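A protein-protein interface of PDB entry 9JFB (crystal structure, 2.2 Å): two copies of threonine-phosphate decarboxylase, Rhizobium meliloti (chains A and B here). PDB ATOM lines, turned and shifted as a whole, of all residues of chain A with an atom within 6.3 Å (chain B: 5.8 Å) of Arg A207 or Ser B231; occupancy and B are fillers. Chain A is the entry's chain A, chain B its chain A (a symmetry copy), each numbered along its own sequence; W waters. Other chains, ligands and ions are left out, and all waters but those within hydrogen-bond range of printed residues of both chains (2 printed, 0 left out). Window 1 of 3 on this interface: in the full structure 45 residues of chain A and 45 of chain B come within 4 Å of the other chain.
Arg A207 touches Val B230, and with the chains exchanged Val A230 touches Arg B207. Arg A207 touches Ser B231, and with the chains exchanged Ser A231 touches Arg B207. 6 positions are printed for both chains. Of the 12 pairs that touch across the chains among the printed residues, 4 have their exchanged pair printed and touching as well.
N of Ala B234 lies within hydrogen-bond range of OG of Ser B231. O of Gly B232 is in hydrogen-bond range of OG1 of Thr B236, 2.8 Å away. The side-chain hydroxyl (OG) of Ser A231 lies within hydrogen-bond range of the backbone NH (N) of Ala A234, 3.0 Å away. O of Ala A204 is in hydrogen-bond range of NH1 of Arg A207 (3.0 Å). N of Gly A79 sits at hydrogen-bond distance from O of Arg A207.
Arg A207 touches just these residues of chain B: Leu B50, Trp B228, Val B230 and Ser B231. Of chain A, only Gly A205 and Arg A207 come within 4 Å of Ser B231. Of the printed residues of chain A, Arg B207 touches Val A230 (3.98 Å) and Ser A231 (3.7 Å). Of the printed residues of chain A, Pro B51 touches Ala A204 (3.7 Å). Leu B206 touches none of the printed residues of chain A. The nearest residue of chain A that does not touch Ser B231 is Leu A206 (4.4 Å). The nearest printed residue of chain A that does not touch Gly B232 is Leu A206 (5.0 Å).
Among the printed residues, merely in contact across the chains: Gly A205 with Ser B231, Gly A205 with Pro B233, Ala A204 with Leu B50, Ser A231 with Arg B207, Arg A207 with Ser B231, Arg A207 with Leu B50, Ala A204 with Pro B51, Gln A81 with Pro B227, Val A230 with Arg B207 and Arg A207 with Val B230.
Printed residues of chain B that touch a printed residue of chain A: Leu B50, Pro B51, Arg B207, Pro B227, Trp B228, Val B230, Ser B231, Gly B232 and Pro B233. Hydrophobic or aromatic side chains of chain B within 4 Å of the printed part of chain A: Leu B50, Pro B51, Pro B227, Trp B228 and Pro B233. Printed residues of chain A that touch a printed residue of chain B: Gln A81, Ala A204, Gly A205, Arg A207, Val A230 and Ser A231. Hydrophobic or aromatic side chains of chain A that line the printed part of chain B: Ala A204. Among the printed residues, no Asp or Glu carboxylate lies within 4 Å of a Lys or Arg side-chain nitrogen of the other chain.
Water W2 bridges the backbone carbonyl oxygen of Ala B229 (2.7 Å) and the backbone carbonyl oxygen of Pro A78 (2.7 Å). Water W1 lies within hydrogen-bond range of NH2 of Arg A207 (2.7 Å), O of Pro B227 (3.0 Å) and O of Trp B228 (3.1 Å).
The guanidinium group of Arg A207 sits at hydrogen-bond distance from the backbone carbonyl oxygen of Trp B228, at 2.9 Å. N of Gly B232 sits at hydrogen-bond distance from O of Gly A205.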
ATOM      1  N   VAL A  77      -8.043 -17.165   1.565  1.00  0.00           N
ATOM      2  CA  VAL A  77      -6.955 -16.387   0.964  1.00  0.00           C
ATOM      3  C   VAL A  77      -7.449 -15.791  -0.338  1.00  0.00           C
ATOM      4  O   VAL A  77      -8.398 -16.296  -0.952  1.00  0.00           O
ATOM      5  CB  VAL A  77      -5.701 -17.261   0.714  1.00  0.00           C
ATOM      6  CG1 VAL A  77      -5.225 -17.878   2.029  1.00  0.00           C
ATOM      7  CG2 VAL A  77      -6.002 -18.407  -0.301  1.00  0.00           C
ATOM      8  N   PRO A  78      -6.872 -14.679  -0.763  1.00  0.00           N
ATOM      9  CA  PRO A  78      -7.457 -13.982  -1.924  1.00  0.00           C
ATOM     10  C   PRO A  78      -7.041 -14.605  -3.257  1.00  0.00           C
ATOM     11  O   PRO A  78      -6.394 -13.970  -4.092  1.00  0.00           O
ATOM     12  CB  PRO A  78      -6.927 -12.555  -1.750  1.00  0.00           C
ATOM     13  CG  PRO A  78      -5.567 -12.755  -1.078  1.00  0.00           C
ATOM     14  CD  PRO A  78      -5.747 -13.929  -0.154  1.00  0.00           C
ATOM     15  N   GLY A  79      -7.441 -15.851  -3.474  1.00  0.00           N
ATOM     16  CA  GLY A  79      -6.984 -16.549  -4.666  1.00  0.00           C
ATOM     17  C   GLY A  79      -5.750 -17.386  -4.393  1.00  0.00           C
ATOM     18  O   GLY A  79      -4.872 -17.029  -3.604  1.00  0.00           O
ATOM     19  N   THR A  80      -5.696 -18.543  -5.055  1.00  0.00           N
ATOM     20  CA  THR A  80      -4.598 -19.482  -4.839  1.00  0.00           C
ATOM     21  C   THR A  80      -3.233 -18.871  -5.186  1.00  0.00           C
ATOM     22  O   THR A  80      -2.236 -19.161  -4.506  1.00  0.00           O
ATOM     23  CB  THR A  80      -4.849 -20.760  -5.647  1.00  0.00           C
ATOM     24  OG1 THR A  80      -6.036 -21.408  -5.146  1.00  0.00           O
ATOM     25  CG2 THR A  80      -3.665 -21.731  -5.511  1.00  0.00           C
ATOM     26  N   GLN A  81      -3.159 -18.025  -6.220  1.00  0.00           N
ATOM     27  CA  GLN A  81      -1.878 -17.400  -6.565  1.00  0.00           C
ATOM     28  C   GLN A  81      -1.258 -16.677  -5.378  1.00  0.00           C
ATOM     29  O   GLN A  81      -0.028 -16.678  -5.211  1.00  0.00           O
ATOM     30  CB  GLN A  81      -2.041 -16.405  -7.716  1.00  0.00           C
ATOM     31  CG  GLN A  81      -0.699 -15.775  -8.160  1.00  0.00           C
ATOM     32  CD  GLN A  81       0.229 -16.774  -8.872  1.00  0.00           C
ATOM     33  OE1 GLN A  81      -0.217 -17.800  -9.377  1.00  0.00           O
ATOM     34  NE2 GLN A  81       1.519 -16.463  -8.922  1.00  0.00           N
ATOM     35  N   GLY A 198     -13.278 -20.515  -7.366  1.00  0.00           N
ATOM     36  CA  GLY A 198     -13.895 -20.039  -8.593  1.00  0.00           C
ATOM     37  C   GLY A 198     -14.257 -21.143  -9.574  1.00  0.00           C
ATOM     38  O   GLY A 198     -15.285 -21.066 -10.245  1.00  0.00           O
ATOM     39  N   LEU A 203     -17.486 -18.947 -10.449  1.00  0.00           N
ATOM     40  CA  LEU A 203     -17.447 -17.542 -10.058  1.00  0.00           C
ATOM     41  C   LEU A 203     -15.993 -17.120  -9.867  1.00  0.00           C
ATOM     42  O   LEU A 203     -15.591 -16.657  -8.803  1.00  0.00           O
ATOM     43  CB  LEU A 203     -18.263 -17.306  -8.792  1.00  0.00           C
ATOM     44  CG  LEU A 203     -19.752 -17.611  -8.935  1.00  0.00           C
ATOM     45  CD1 LEU A 203     -20.372 -17.703  -7.572  1.00  0.00           C
ATOM     46  CD2 LEU A 203     -20.445 -16.551  -9.786  1.00  0.00           C
ATOM     47  N   ALA A 204     -15.192 -17.302 -10.916  1.00  0.00           N
ATOM     48  CA  ALA A 204     -13.773 -16.979 -10.864  1.00  0.00           C
ATOM     49  C   ALA A 204     -13.506 -15.480 -10.925  1.00  0.00           C
ATOM     50  O   ALA A 204     -12.346 -15.069 -10.832  1.00  0.00           O
ATOM     51  CB  ALA A 204     -13.041 -17.692 -12.006  1.00  0.00           C
ATOM     52  N   GLY A 205     -14.540 -14.662 -11.118  1.00  0.00           N
ATOM     53  CA  GLY A 205     -14.377 -13.229 -10.944  1.00  0.00           C
ATOM     54  C   GLY A 205     -14.019 -12.865  -9.517  1.00  0.00           C
ATOM     55  O   GLY A 205     -13.267 -11.918  -9.278  1.00  0.00           O
ATOM     56  N   LEU A 206     -14.572 -13.598  -8.552  1.00  0.00           N
ATOM     57  CA  LEU A 206     -14.103 -13.505  -7.181  1.00  0.00           C
ATOM     58  C   LEU A 206     -12.737 -14.157  -7.079  1.00  0.00           C
ATOM     59  O   LEU A 206     -12.446 -15.134  -7.772  1.00  0.00           O
ATOM     60  CB  LEU A 206     -15.076 -14.207  -6.230  1.00  0.00           C
ATOM     61  CG  LEU A 206     -16.476 -13.596  -6.231  1.00  0.00           C
ATOM     62  CD1 LEU A 206     -17.456 -14.484  -5.493  1.00  0.00           C
ATOM     63  CD2 LEU A 206     -16.423 -12.218  -5.610  1.00  0.00           C
ATOM     64  N   ARG A 207     -11.890 -13.622  -6.212  1.00  0.00           N
ATOM     65  CA  ARG A 207     -10.560 -14.199  -6.003  1.00  0.00           C
ATOM     66  C   ARG A 207     -10.542 -14.802  -4.607  1.00  0.00           C
ATOM     67  O   ARG A 207     -10.357 -14.091  -3.610  1.00  0.00           O
ATOM     68  CB  ARG A 207      -9.479 -13.147  -6.202  1.00  0.00           C
ATOM     69  CG  ARG A 207      -9.696 -12.340  -7.496  1.00  0.00           C
ATOM     70  CD  ARG A 207      -9.831 -13.237  -8.744  1.00  0.00           C
ATOM     71  NE  ARG A 207      -8.698 -14.152  -8.900  1.00  0.00           N
ATOM     72  CZ  ARG A 207      -8.810 -15.463  -9.085  1.00  0.00           C
ATOM     73  NH1 ARG A 207      -9.994 -16.044  -9.242  1.00  0.00           N
ATOM     74  NH2 ARG A 207      -7.707 -16.209  -9.127  1.00  0.00           N
ATOM     75  N   LEU A 208     -10.729 -16.116  -4.537  1.00  0.00           N
ATOM     76  CA  LEU A 208     -10.898 -16.785  -3.255  1.00  0.00           C
ATOM     77  C   LEU A 208     -10.343 -18.201  -3.311  1.00  0.00           C
ATOM     78  O   LEU A 208     -10.666 -18.971  -4.221  1.00  0.00           O
ATOM     79  CB  LEU A 208     -12.375 -16.831  -2.850  1.00  0.00           C
ATOM     80  CG  LEU A 208     -12.624 -17.551  -1.520  1.00  0.00           C
ATOM     81  CD1 LEU A 208     -11.952 -16.813  -0.336  1.00  0.00           C
ATOM     82  CD2 LEU A 208     -14.109 -17.693  -1.287  1.00  0.00           C
ATOM     83  N   GLY A 209      -9.514 -18.534  -2.326  1.00  0.00           N
ATOM     84  CA  GLY A 209      -9.058 -19.891  -2.111  1.00  0.00           C
ATOM     85  C   GLY A 209      -9.065 -20.186  -0.623  1.00  0.00           C
ATOM     86  O   GLY A 209      -9.372 -19.319   0.194  1.00  0.00           O
ATOM     87  N   ALA A 229      -7.382  -9.383   3.786  1.00  0.00           N
ATOM     88  CA  ALA A 229      -6.854  -9.833   2.499  1.00  0.00           C
ATOM     89  C   ALA A 229      -7.965 -10.267   1.550  1.00  0.00           C
ATOM     90  O   ALA A 229      -7.818 -10.125   0.329  1.00  0.00           O
ATOM     91  CB  ALA A 229      -5.849 -10.965   2.703  1.00  0.00           C
ATOM     92  N   VAL A 230      -9.079 -10.777   2.081  1.00  0.00           N
ATOM     93  CA  VAL A 230     -10.161 -11.360   1.287  1.00  0.00           C
ATOM     94  C   VAL A 230     -11.406 -10.484   1.379  1.00  0.00           C
ATOM     95  O   VAL A 230     -11.813 -10.068   2.473  1.00  0.00           O
ATOM     96  CB  VAL A 230     -10.475 -12.794   1.757  1.00  0.00           C
ATOM     97  CG1 VAL A 230     -11.596 -13.395   0.907  1.00  0.00           C
ATOM     98  CG2 VAL A 230      -9.214 -13.657   1.693  1.00  0.00           C
ATOM     99  N   SER A 231     -12.042 -10.250   0.237  1.00  0.00           N
ATOM    100  CA  SER A 231     -13.170  -9.335   0.191  1.00  0.00           C
ATOM    101  C   SER A 231     -14.367  -9.871   0.981  1.00  0.00           C
ATOM    102  O   SER A 231     -14.573 -11.078   1.111  1.00  0.00           O
ATOM    103  CB  SER A 231     -13.571  -9.069  -1.259  1.00  0.00           C
ATOM    104  OG  SER A 231     -14.590  -9.961  -1.660  1.00  0.00           O
ATOM    105  N   ALA A 234     -16.823 -11.884  -1.249  1.00  0.00           N
ATOM    106  CA  ALA A 234     -16.335 -13.236  -1.496  1.00  0.00           C
ATOM    107  C   ALA A 234     -16.655 -14.157  -0.325  1.00  0.00           C
ATOM    108  O   ALA A 234     -17.148 -15.274  -0.516  1.00  0.00           O
ATOM    109  CB  ALA A 234     -14.826 -13.207  -1.767  1.00  0.00           C
ATOM    110  N   LEU B  50     -12.514 -15.353 -14.818  1.00  0.00           N
ATOM    111  CA  LEU B  50     -11.247 -14.796 -14.379  1.00  0.00           C
ATOM    112  C   LEU B  50     -11.122 -13.379 -14.928  1.00  0.00           C
ATOM    113  O   LEU B  50     -11.477 -13.140 -16.089  1.00  0.00           O
ATOM    114  CB  LEU B  50     -10.076 -15.658 -14.871  1.00  0.00           C
ATOM    115  CG  LEU B  50     -10.014 -17.067 -14.282  1.00  0.00           C
ATOM    116  CD1 LEU B  50      -9.047 -17.932 -15.075  1.00  0.00           C
ATOM    117  CD2 LEU B  50      -9.606 -17.030 -12.797  1.00  0.00           C
ATOM    118  N   PRO B  51     -10.666 -12.419 -14.125  1.00  0.00           N
ATOM    119  CA  PRO B  51     -10.720 -11.008 -14.559  1.00  0.00           C
ATOM    120  C   PRO B  51      -9.918 -10.797 -15.833  1.00  0.00           C
ATOM    121  O   PRO B  51      -8.721 -11.078 -15.887  1.00  0.00           O
ATOM    122  CB  PRO B  51     -10.142 -10.235 -13.360  1.00  0.00           C
ATOM    123  CG  PRO B  51      -9.633 -11.288 -12.389  1.00  0.00           C
ATOM    124  CD  PRO B  51     -10.347 -12.562 -12.698  1.00  0.00           C
ATOM    125  N   LEU B 206     -14.962  -4.435  -0.594  1.00  0.00           N
ATOM    126  CA  LEU B 206     -14.066  -4.693  -1.708  1.00  0.00           C
ATOM    127  C   LEU B 206     -12.644  -4.380  -1.283  1.00  0.00           C
ATOM    128  O   LEU B 206     -12.404  -3.468  -0.490  1.00  0.00           O
ATOM    129  CB  LEU B 206     -14.442  -3.828  -2.913  1.00  0.00           C
ATOM    130  CG  LEU B 206     -15.849  -4.098  -3.443  1.00  0.00           C
ATOM    131  CD1 LEU B 206     -16.265  -3.040  -4.443  1.00  0.00           C
ATOM    132  CD2 LEU B 206     -15.897  -5.477  -4.062  1.00  0.00           C
ATOM    133  N   ARG B 207     -11.691  -5.134  -1.810  1.00  0.00           N
ATOM    134  CA  ARG B 207     -10.279  -4.889  -1.502  1.00  0.00           C
ATOM    135  C   ARG B 207      -9.622  -4.368  -2.771  1.00  0.00           C
ATOM    136  O   ARG B 207      -9.261  -5.146  -3.664  1.00  0.00           O
ATOM    137  CB  ARG B 207      -9.617  -6.153  -0.973  1.00  0.00           C
ATOM    138  CG  ARG B 207     -10.465  -6.831   0.120  1.00  0.00           C
ATOM    139  CD  ARG B 207     -10.829  -5.874   1.273  1.00  0.00           C
ATOM    140  NE  ARG B 207      -9.648  -5.239   1.866  1.00  0.00           N
ATOM    141  CZ  ARG B 207      -9.512  -3.931   2.055  1.00  0.00           C
ATOM    142  NH1 ARG B 207     -10.506  -3.086   1.801  1.00  0.00           N
ATOM    143  NH2 ARG B 207      -8.359  -3.459   2.523  1.00  0.00           N
ATOM    144  N   PRO B 227      -0.978 -13.174 -11.487  1.00  0.00           N
ATOM    145  CA  PRO B 227      -2.186 -13.058 -12.313  1.00  0.00           C
ATOM    146  C   PRO B 227      -3.475 -12.988 -11.497  1.00  0.00           C
ATOM    147  O   PRO B 227      -3.600 -13.591 -10.426  1.00  0.00           O
ATOM    148  CB  PRO B 227      -2.145 -14.333 -13.163  1.00  0.00           C
ATOM    149  CG  PRO B 227      -1.312 -15.309 -12.336  1.00  0.00           C
ATOM    150  CD  PRO B 227      -0.255 -14.441 -11.726  1.00  0.00           C
ATOM    151  N   TRP B 228      -4.451 -12.243 -12.039  1.00  0.00           N
ATOM    152  CA  TRP B 228      -5.811 -12.186 -11.487  1.00  0.00           C
ATOM    153  C   TRP B 228      -5.810 -11.737 -10.022  1.00  0.00           C
ATOM    154  O   TRP B 228      -6.512 -12.304  -9.181  1.00  0.00           O
ATOM    155  CB  TRP B 228      -6.518 -13.543 -11.615  1.00  0.00           C
ATOM    156  CG  TRP B 228      -6.391 -14.220 -12.943  1.00  0.00           C
ATOM    157  CD1 TRP B 228      -6.857 -13.770 -14.150  1.00  0.00           C
ATOM    158  CD2 TRP B 228      -5.770 -15.489 -13.199  1.00  0.00           C
ATOM    159  NE1 TRP B 228      -6.546 -14.680 -15.142  1.00  0.00           N
ATOM    160  CE2 TRP B 228      -5.895 -15.747 -14.579  1.00  0.00           C
ATOM    161  CE3 TRP B 228      -5.129 -16.436 -12.392  1.00  0.00           C
ATOM    162  CZ2 TRP B 228      -5.398 -16.910 -15.168  1.00  0.00           C
ATOM    163  CZ3 TRP B 228      -4.633 -17.587 -12.974  1.00  0.00           C
ATOM    164  CH2 TRP B 228      -4.772 -17.816 -14.351  1.00  0.00           C
ATOM    165  N   ALA B 229      -5.000 -10.732  -9.694  1.00  0.00           N
ATOM    166  CA  ALA B 229      -4.882 -10.361  -8.285  1.00  0.00           C
ATOM    167  C   ALA B 229      -6.128  -9.641  -7.781  1.00  0.00           C
ATOM    168  O   ALA B 229      -6.466  -9.759  -6.596  1.00  0.00           O
ATOM    169  CB  ALA B 229      -3.639  -9.501  -8.065  1.00  0.00           C
ATOM    170  N   VAL B 230      -6.826  -8.911  -8.654  1.00  0.00           N
ATOM    171  CA  VAL B 230      -7.954  -8.059  -8.277  1.00  0.00           C
ATOM    172  C   VAL B 230      -9.250  -8.627  -8.849  1.00  0.00           C
ATOM    173  O   VAL B 230      -9.321  -8.985 -10.034  1.00  0.00           O
ATOM    174  CB  VAL B 230      -7.738  -6.614  -8.766  1.00  0.00           C
ATOM    175  CG1 VAL B 230      -8.918  -5.733  -8.350  1.00  0.00           C
ATOM    176  CG2 VAL B 230      -6.421  -6.064  -8.215  1.00  0.00           C
ATOM    177  N   SER B 231     -10.289  -8.657  -8.023  1.00  0.00           N
ATOM    178  CA  SER B 231     -11.537  -9.284  -8.426  1.00  0.00           C
ATOM    179  C   SER B 231     -12.211  -8.521  -9.569  1.00  0.00           C
ATOM    180  O   SER B 231     -12.072  -7.305  -9.712  1.00  0.00           O
ATOM    181  CB  SER B 231     -12.482  -9.386  -7.230  1.00  0.00           C
ATOM    182  OG  SER B 231     -13.341  -8.266  -7.183  1.00  0.00           O
ATOM    183  N   GLY B 232     -12.946  -9.261 -10.398  1.00  0.00           N
ATOM    184  CA  GLY B 232     -13.700  -8.676 -11.485  1.00  0.00           C
ATOM    185  C   GLY B 232     -14.774  -7.700 -11.031  1.00  0.00           C
ATOM    186  O   GLY B 232     -14.925  -6.609 -11.594  1.00  0.00           O
ATOM    187  N   PRO B 233     -15.567  -8.085 -10.026  1.00  0.00           N
ATOM    188  CA  PRO B 233     -16.531  -7.122  -9.467  1.00  0.00           C
ATOM    189  C   PRO B 233     -15.888  -5.825  -9.007  1.00  0.00           C
ATOM    190  O   PRO B 233     -16.407  -4.747  -9.306  1.00  0.00           O
ATOM    191  CB  PRO B 233     -17.164  -7.906  -8.303  1.00  0.00           C
ATOM    192  CG  PRO B 233     -17.152  -9.296  -8.755  1.00  0.00           C
ATOM    193  CD  PRO B 233     -15.818  -9.450  -9.522  1.00  0.00           C
ATOM    194  N   ALA B 234     -14.767  -5.899  -8.286  1.00  0.00           N
ATOM    195  CA  ALA B 234     -14.103  -4.687  -7.820  1.00  0.00           C
ATOM    196  C   ALA B 234     -13.758  -3.769  -8.987  1.00  0.00           C
ATOM    197  O   ALA B 234     -14.015  -2.561  -8.938  1.00  0.00           O
ATOM    198  CB  ALA B 234     -12.843  -5.052  -7.027  1.00  0.00           C
ATOM    199  N   LEU B 235     -13.172  -4.333 -10.050  1.00  0.00           N
ATOM    200  CA  LEU B 235     -12.739  -3.539 -11.200  1.00  0.00           C
ATOM    201  C   LEU B 235     -13.928  -2.935 -11.950  1.00  0.00           C
ATOM    202  O   LEU B 235     -13.875  -1.781 -12.393  1.00  0.00           O
ATOM    203  CB  LEU B 235     -11.896  -4.422 -12.130  1.00  0.00           C
ATOM    204  CG  LEU B 235     -10.581  -4.991 -11.565  1.00  0.00           C
ATOM    205  CD1 LEU B 235     -10.063  -6.165 -12.398  1.00  0.00           C
ATOM    206  CD2 LEU B 235      -9.520  -3.891 -11.509  1.00  0.00           C
ATOM    207  N   THR B 236     -15.015  -3.697 -12.080  1.00  0.00           N
ATOM    208  CA  THR B 236     -16.233  -3.184 -12.704  1.00  0.00           C
ATOM    209  C   THR B 236     -16.806  -2.014 -11.904  1.00  0.00           C
ATOM    210  O   THR B 236     -17.128  -0.945 -12.457  1.00  0.00           O
ATOM    211  CB  THR B 236     -17.258  -4.326 -12.808  1.00  0.00           C
ATOM    212  OG1 THR B 236     -16.645  -5.458 -13.444  1.00  0.00           O
ATOM    213  CG2 THR B 236     -18.473  -3.903 -13.617  1.00  0.00           C
HETATM  214  O   HOH W   1      -5.296 -15.087  -8.443  1.00  0.00           O
HETATM  215  O   HOH W   2      -5.676 -11.391  -4.649  1.00  0.00           O
